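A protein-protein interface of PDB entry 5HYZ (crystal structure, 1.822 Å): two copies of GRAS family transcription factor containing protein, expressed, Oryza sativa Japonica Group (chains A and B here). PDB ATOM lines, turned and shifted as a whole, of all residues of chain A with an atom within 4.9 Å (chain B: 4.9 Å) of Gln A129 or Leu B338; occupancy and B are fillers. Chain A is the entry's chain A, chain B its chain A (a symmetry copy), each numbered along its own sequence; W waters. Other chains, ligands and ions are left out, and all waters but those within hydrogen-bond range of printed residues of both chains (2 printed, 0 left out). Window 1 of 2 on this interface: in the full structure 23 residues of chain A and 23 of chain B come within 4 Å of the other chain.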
ATOM      1  N   ILE A 122     -21.750  15.643   9.443  1.00  0.00           N
ATOM      2  CA  ILE A 122     -23.128  15.457   8.895  1.00  0.00           C
ATOM      3  C   ILE A 122     -23.164  15.345   7.371  1.00  0.00           C
ATOM      4  O   ILE A 122     -23.975  14.574   6.832  1.00  0.00           O
ATOM      5  CB  ILE A 122     -24.062  16.579   9.406  1.00  0.00           C
ATOM      6  CG1 ILE A 122     -25.535  16.138   9.149  1.00  0.00           C
ATOM      7  CG2 ILE A 122     -23.718  17.869   8.744  1.00  0.00           C
ATOM      8  CD1 ILE A 122     -26.613  17.042   9.783  1.00  0.00           C
ATOM      9  N   ALA A 125     -22.529  11.681   6.805  1.00  0.00           N
ATOM     10  CA  ALA A 125     -23.642  10.819   7.226  1.00  0.00           C
ATOM     11  C   ALA A 125     -24.754  10.871   6.156  1.00  0.00           C
ATOM     12  O   ALA A 125     -25.286   9.833   5.743  1.00  0.00           O
ATOM     13  CB  ALA A 125     -24.170  11.269   8.580  1.00  0.00           C
ATOM     14  N   ALA A 126     -25.006  12.080   5.648  1.00  0.00           N
ATOM     15  CA  ALA A 126     -25.990  12.209   4.577  1.00  0.00           C
ATOM     16  C   ALA A 126     -25.564  11.443   3.320  1.00  0.00           C
ATOM     17  O   ALA A 126     -26.383  10.760   2.630  1.00  0.00           O
ATOM     18  CB  ALA A 126     -26.242  13.731   4.288  1.00  0.00           C
ATOM     19  N   LEU A 127     -24.282  11.558   2.961  1.00  0.00           N
ATOM     20  CA  LEU A 127     -23.823  10.873   1.782  1.00  0.00           C
ATOM     21  C   LEU A 127     -23.884   9.344   1.969  1.00  0.00           C
ATOM     22  O   LEU A 127     -24.234   8.612   1.058  1.00  0.00           O
ATOM     23  CB  LEU A 127     -22.338  11.269   1.453  1.00  0.00           C
ATOM     24  CG  LEU A 127     -21.890  10.587   0.143  1.00  0.00           C
ATOM     25  CD1 LEU A 127     -22.487  11.267  -1.132  1.00  0.00           C
ATOM     26  CD2 LEU A 127     -20.354  10.641  -0.026  1.00  0.00           C
ATOM     27  N   LEU A 128     -23.509   8.869   3.142  1.00  0.00           N
ATOM     28  CA  LEU A 128     -23.574   7.409   3.387  1.00  0.00           C
ATOM     29  C   LEU A 128     -25.014   6.903   3.193  1.00  0.00           C
ATOM     30  O   LEU A 128     -25.265   5.886   2.557  1.00  0.00           O
ATOM     31  CB  LEU A 128     -23.104   7.110   4.807  1.00  0.00           C
ATOM     32  CG  LEU A 128     -21.559   7.165   4.969  1.00  0.00           C
ATOM     33  CD1 LEU A 128     -21.163   7.123   6.498  1.00  0.00           C
ATOM     34  CD2 LEU A 128     -20.918   6.023   4.168  1.00  0.00           C
ATOM     35  N   GLN A 129     -25.949   7.619   3.782  1.00  0.00           N
ATOM     36  CA  GLN A 129     -27.366   7.231   3.587  1.00  0.00           C
ATOM     37  C   GLN A 129     -27.762   7.195   2.109  1.00  0.00           C
ATOM     38  O   GLN A 129     -28.413   6.226   1.594  1.00  0.00           O
ATOM     39  CB  GLN A 129     -28.242   8.209   4.357  1.00  0.00           C
ATOM     40  CG  GLN A 129     -29.813   7.949   4.213  1.00  0.00           C
ATOM     41  CD  GLN A 129     -30.240   6.742   4.999  1.00  0.00           C
ATOM     42  OE1 GLN A 129     -29.555   6.298   5.910  1.00  0.00           O
ATOM     43  NE2 GLN A 129     -31.413   6.181   4.642  1.00  0.00           N
ATOM     44  N   ALA A 130     -27.336   8.239   1.387  1.00  0.00           N
ATOM     45  CA  ALA A 130     -27.625   8.293  -0.048  1.00  0.00           C
ATOM     46  C   ALA A 130     -26.955   7.183  -0.847  1.00  0.00           C
ATOM     47  O   ALA A 130     -27.594   6.579  -1.700  1.00  0.00           O
ATOM     48  CB  ALA A 130     -27.242   9.693  -0.612  1.00  0.00           C
ATOM     49  N   LEU A 131     -25.678   6.881  -0.571  1.00  0.00           N
ATOM     50  CA  LEU A 131     -24.966   5.812  -1.246  1.00  0.00           C
ATOM     51  C   LEU A 131     -25.648   4.471  -0.976  1.00  0.00           C
ATOM     52  O   LEU A 131     -25.679   3.603  -1.853  1.00  0.00           O
ATOM     53  CB  LEU A 131     -23.467   5.738  -0.770  1.00  0.00           C
ATOM     54  CG  LEU A 131     -22.609   6.917  -1.296  1.00  0.00           C
ATOM     55  CD1 LEU A 131     -21.240   7.002  -0.572  1.00  0.00           C
ATOM     56  CD2 LEU A 131     -22.440   6.770  -2.795  1.00  0.00           C
ATOM     57  N   ALA A 132     -26.192   4.319   0.232  1.00  0.00           N
ATOM     58  CA  ALA A 132     -26.751   3.010   0.589  1.00  0.00           C
ATOM     59  C   ALA A 132     -27.947   2.762  -0.253  1.00  0.00           C
ATOM     60  O   ALA A 132     -28.248   1.605  -0.550  1.00  0.00           O
ATOM     61  CB  ALA A 132     -27.112   2.926   2.068  1.00  0.00           C
ATOM     62  N   THR A 133     -28.639   3.841  -0.623  1.00  0.00           N
ATOM     63  CA  THR A 133     -29.823   3.660  -1.450  1.00  0.00           C
ATOM     64  C   THR A 133     -29.697   4.067  -2.948  1.00  0.00           C
ATOM     65  O   THR A 133     -30.703   4.263  -3.651  1.00  0.00           O
ATOM     66  CB  THR A 133     -31.017   4.423  -0.793  1.00  0.00           C
ATOM     67  OG1 THR A 133     -30.643   5.773  -0.506  1.00  0.00           O
ATOM     68  CG2 THR A 133     -31.323   3.796   0.554  1.00  0.00           C
ATOM     69  N   PHE A 170     -22.629   4.988  12.478  1.00  0.00           N
ATOM     70  CA  PHE A 170     -23.690   5.132  11.457  1.00  0.00           C
ATOM     71  C   PHE A 170     -23.568   4.152  10.312  1.00  0.00           C
ATOM     72  O   PHE A 170     -24.553   3.518   9.828  1.00  0.00           O
ATOM     73  CB  PHE A 170     -23.641   6.593  10.944  1.00  0.00           C
ATOM     74  CG  PHE A 170     -24.814   6.975  10.051  1.00  0.00           C
ATOM     75  CD1 PHE A 170     -26.038   7.244  10.614  1.00  0.00           C
ATOM     76  CD2 PHE A 170     -24.658   7.071   8.654  1.00  0.00           C
ATOM     77  CE1 PHE A 170     -27.117   7.577   9.825  1.00  0.00           C
ATOM     78  CE2 PHE A 170     -25.771   7.389   7.843  1.00  0.00           C
ATOM     79  CZ  PHE A 170     -26.980   7.671   8.462  1.00  0.00           C
ATOM     80  N   LEU A 174     -25.879   0.909   8.297  1.00  0.00           N
ATOM     81  CA  LEU A 174     -26.102   0.655   6.872  1.00  0.00           C
ATOM     82  C   LEU A 174     -25.562  -0.635   6.321  1.00  0.00           C
ATOM     83  O   LEU A 174     -25.759  -0.915   5.139  1.00  0.00           O
ATOM     84  CB  LEU A 174     -25.467   1.797   6.027  1.00  0.00           C
ATOM     85  CG  LEU A 174     -25.875   3.214   6.433  1.00  0.00           C
ATOM     86  CD1 LEU A 174     -24.867   4.225   5.782  1.00  0.00           C
ATOM     87  CD2 LEU A 174     -27.296   3.533   6.000  1.00  0.00           C
ATOM     88  N   TYR B 331     -32.889   0.675   6.188  1.00  0.00           N
ATOM     89  CA  TYR B 331     -32.362   2.019   6.284  1.00  0.00           C
ATOM     90  C   TYR B 331     -33.321   3.025   6.941  1.00  0.00           C
ATOM     91  O   TYR B 331     -33.190   4.228   6.742  1.00  0.00           O
ATOM     92  CB  TYR B 331     -31.999   2.526   4.883  1.00  0.00           C
ATOM     93  CG  TYR B 331     -31.146   1.512   4.141  1.00  0.00           C
ATOM     94  CD1 TYR B 331     -29.895   1.129   4.639  1.00  0.00           C
ATOM     95  CD2 TYR B 331     -31.608   0.908   3.008  1.00  0.00           C
ATOM     96  CE1 TYR B 331     -29.118   0.139   3.991  1.00  0.00           C
ATOM     97  CE2 TYR B 331     -30.831  -0.064   2.342  1.00  0.00           C
ATOM     98  CZ  TYR B 331     -29.596  -0.443   2.842  1.00  0.00           C
ATOM     99  OH  TYR B 331     -28.792  -1.408   2.214  1.00  0.00           O
ATOM    100  N   SER B 334     -31.246   4.202  10.181  1.00  0.00           N
ATOM    101  CA  SER B 334     -30.193   5.123   9.808  1.00  0.00           C
ATOM    102  C   SER B 334     -30.836   6.447   9.355  1.00  0.00           C
ATOM    103  O   SER B 334     -30.321   7.519   9.659  1.00  0.00           O
ATOM    104  CB  SER B 334     -29.290   4.558   8.681  1.00  0.00           C
ATOM    105  OG  SER B 334     -30.085   4.007   7.631  1.00  0.00           O
ATOM    106  N   GLN B 335     -31.900   6.393   8.594  1.00  0.00           N
ATOM    107  CA  GLN B 335     -32.491   7.666   8.134  1.00  0.00           C
ATOM    108  C   GLN B 335     -32.972   8.515   9.313  1.00  0.00           C
ATOM    109  O   GLN B 335     -32.840   9.755   9.368  1.00  0.00           O
ATOM    110  CB  GLN B 335     -33.651   7.419   7.216  1.00  0.00           C
ATOM    111  CG  GLN B 335     -34.316   8.688   6.823  1.00  0.00           C
ATOM    112  CD  GLN B 335     -35.435   8.422   5.889  1.00  0.00           C
ATOM    113  OE1 GLN B 335     -35.404   8.880   4.745  1.00  0.00           O
ATOM    114  NE2 GLN B 335     -36.471   7.674   6.371  1.00  0.00           N
ATOM    115  N   ALA B 336     -33.528   7.825  10.291  1.00  0.00           N
ATOM    116  CA  ALA B 336     -33.948   8.550  11.500  1.00  0.00           C
ATOM    117  C   ALA B 336     -32.793   9.070  12.347  1.00  0.00           C
ATOM    118  O   ALA B 336     -32.872  10.179  12.860  1.00  0.00           O
ATOM    119  CB  ALA B 336     -34.902   7.640  12.338  1.00  0.00           C
ATOM    120  N   ASP B 337     -31.675   8.330  12.452  1.00  0.00           N
ATOM    121  CA  ASP B 337     -30.465   8.881  13.054  1.00  0.00           C
ATOM    122  C   ASP B 337     -29.895  10.044  12.318  1.00  0.00           C
ATOM    123  O   ASP B 337     -29.414  10.993  12.907  1.00  0.00           O
ATOM    124  CB  ASP B 337     -29.401   7.794  13.159  1.00  0.00           C
ATOM    125  CG  ASP B 337     -29.331   7.189  14.544  1.00  0.00           C
ATOM    126  OD1 ASP B 337     -30.130   7.587  15.433  1.00  0.00           O
ATOM    127  OD2 ASP B 337     -28.473   6.309  14.758  1.00  0.00           O
ATOM    128  N   LEU B 338     -29.979  10.009  10.994  1.00  0.00           N
ATOM    129  CA  LEU B 338     -29.484  11.118  10.222  1.00  0.00           C
ATOM    130  C   LEU B 338     -30.297  12.356  10.547  1.00  0.00           C
ATOM    131  O   LEU B 338     -29.777  13.462  10.713  1.00  0.00           O
ATOM    132  CB  LEU B 338     -29.557  10.789   8.724  1.00  0.00           C
ATOM    133  CG  LEU B 338     -29.202  11.917   7.776  1.00  0.00           C
ATOM    134  CD1 LEU B 338     -27.818  12.526   8.091  1.00  0.00           C
ATOM    135  CD2 LEU B 338     -29.280  11.514   6.288  1.00  0.00           C
ATOM    136  N   LEU B 339     -31.618  12.190  10.653  1.00  0.00           N
ATOM    137  CA  LEU B 339     -32.453  13.344  10.906  1.00  0.00           C
ATOM    138  C   LEU B 339     -32.085  13.954  12.262  1.00  0.00           C
ATOM    139  O   LEU B 339     -32.116  15.165  12.443  1.00  0.00           O
ATOM    140  CB  LEU B 339     -33.941  12.873  10.856  1.00  0.00           C
ATOM    141  CG  LEU B 339     -34.789  13.779  11.717  1.00  0.00           C
ATOM    142  CD1 LEU B 339     -34.976  15.068  10.923  1.00  0.00           C
ATOM    143  CD2 LEU B 339     -36.090  13.091  12.075  1.00  0.00           C
ATOM    144  N   LEU B 340     -31.656  13.120  13.202  1.00  0.00           N
ATOM    145  CA  LEU B 340     -31.413  13.591  14.556  1.00  0.00           C
ATOM    146  C   LEU B 340     -29.973  14.102  14.745  1.00  0.00           C
ATOM    147  O   LEU B 340     -29.591  14.527  15.844  1.00  0.00           O
ATOM    148  CB  LEU B 340     -31.689  12.454  15.565  1.00  0.00           C
ATOM    149  CG  LEU B 340     -33.161  11.990  15.698  1.00  0.00           C
ATOM    150  CD1 LEU B 340     -33.273  10.795  16.642  1.00  0.00           C
ATOM    151  CD2 LEU B 340     -34.053  13.165  16.164  1.00  0.00           C
ATOM    152  N   TRP B 341     -29.176  14.032  13.682  1.00  0.00           N
ATOM    153  CA  TRP B 341     -27.729  14.246  13.816  1.00  0.00           C
ATOM    154  C   TRP B 341     -27.376  15.551  14.490  1.00  0.00           C
ATOM    155  O   TRP B 341     -26.475  15.587  15.336  1.00  0.00           O
ATOM    156  CB  TRP B 341     -27.054  14.203  12.442  1.00  0.00           C
ATOM    157  CG  TRP B 341     -25.557  14.054  12.462  1.00  0.00           C
ATOM    158  CD1 TRP B 341     -24.640  15.057  12.521  1.00  0.00           C
ATOM    159  CD2 TRP B 341     -24.803  12.817  12.336  1.00  0.00           C
ATOM    160  NE1 TRP B 341     -23.360  14.522  12.470  1.00  0.00           N
ATOM    161  CE2 TRP B 341     -23.436  13.163  12.323  1.00  0.00           C
ATOM    162  CE3 TRP B 341     -25.161  11.477  12.232  1.00  0.00           C
ATOM    163  CZ2 TRP B 341     -22.417  12.211  12.219  1.00  0.00           C
ATOM    164  CZ3 TRP B 341     -24.143  10.529  12.126  1.00  0.00           C
ATOM    165  CH2 TRP B 341     -22.810  10.894  12.136  1.00  0.00           C
HETATM  166  O   HOH W   1     -33.132   8.091   3.043  1.00  0.00           O
HETATM  167  O   HOH W   2     -29.196  -1.029  -0.370  1.00  0.00           O
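NE2 of Gln A129 sits at hydrogen-bond distance from O of Tyr B331. The side-chain hydroxyl (OG) of Ser B334 is in hydrogen-bond range of the side-chain amide oxygen (OE1) of Gln A129 (2.9 Å).
The side-chain hydroxyl (OG1) of Thr A133 is in hydrogen-bond range of the backbone carbonyl oxygen (O) of Gln A129 (3.1 Å). O of Ala A130 is in hydrogen-bond range of OG1 of Thr A133 (3.4 Å). O of Tyr B331 sits at hydrogen-bond distance from OG of Ser B334 (3.2 Å).
Ile A122 touches Trp B341. Ala A125 touches Leu B338. Ala A125 touches Trp B341. CD1 of Leu B338 touches N of Ala A126, at 3.8 Å. CB of Gln A129 touches CD2 of Leu B338, at 3.97 Å. Tyr B331 touches Ala A132 (CE1 to CB, 3.9 Å). Tyr B331 touches Thr A133 (CD2 to CG2, 3.8 Å). Phe A170 touches Ser B334 (CE1 to O, 3.2 Å). Leu B338 touches Phe A170 (N to CE1, 3.9 Å). Leu A174 touches Ser B334 (CD2 to OG, 3.3 Å).
Printed residues of chain B within 4 Å of Ala A125: Leu B338 (3.9 Å) and Trp B341 (3.6 Å). Leu A127 touches none of the printed residues of chain B. Of the printed residues of chain B, Gln A129 touches Tyr B331 (3.4 Å), Ser B334 (2.9 Å), Gln B335 (3.6 Å) and Leu B338 (3.97 Å). Of the printed residues of chain B, Ala A132 touches Tyr B331 (3.9 Å). Printed residues of chain B within 4 Å of Phe A170: Ser B334 and Leu B338. Of the printed residues of chain B, Leu A174 touches Tyr B331 and Ser B334. Leu B338 touches four residues of chain A. The nearest residue of chain A that does not touch Leu B338 is Ile A122 (4.4 Å).
Of the 9 printed residues of chain B, 5 touch a printed residue of chain A. Printed residues of chain B that touch a printed residue of chain A: Tyr B331, Ser B334, Gln B335, Leu B338 and Trp B341. Along chain B the printed residues that touch a printed residue of chain A span positions 331 to 341. Of the 12 printed residues of chain A, 8 touch a printed residue of chain B. Hydrophobic or aromatic side chains of chain A within 4 Å of the printed part of chain B: Ile A122, Ala A125, Ala A132, Phe A170 and Leu A174. Among the printed residues, 14 pairs touch across the chains.
No position is printed for both chains. Of the 14 pairs that touch across the chains among the printed residues, none has its exchanged pair printed and touching as well.
Water W2 bridges OH of Tyr B331 and O of Ala A132. Water W1 lies within hydrogen-bond range of OE1 of Gln B335 (2.9 Å) and NE2 of Gln A129 (3.0 Å).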
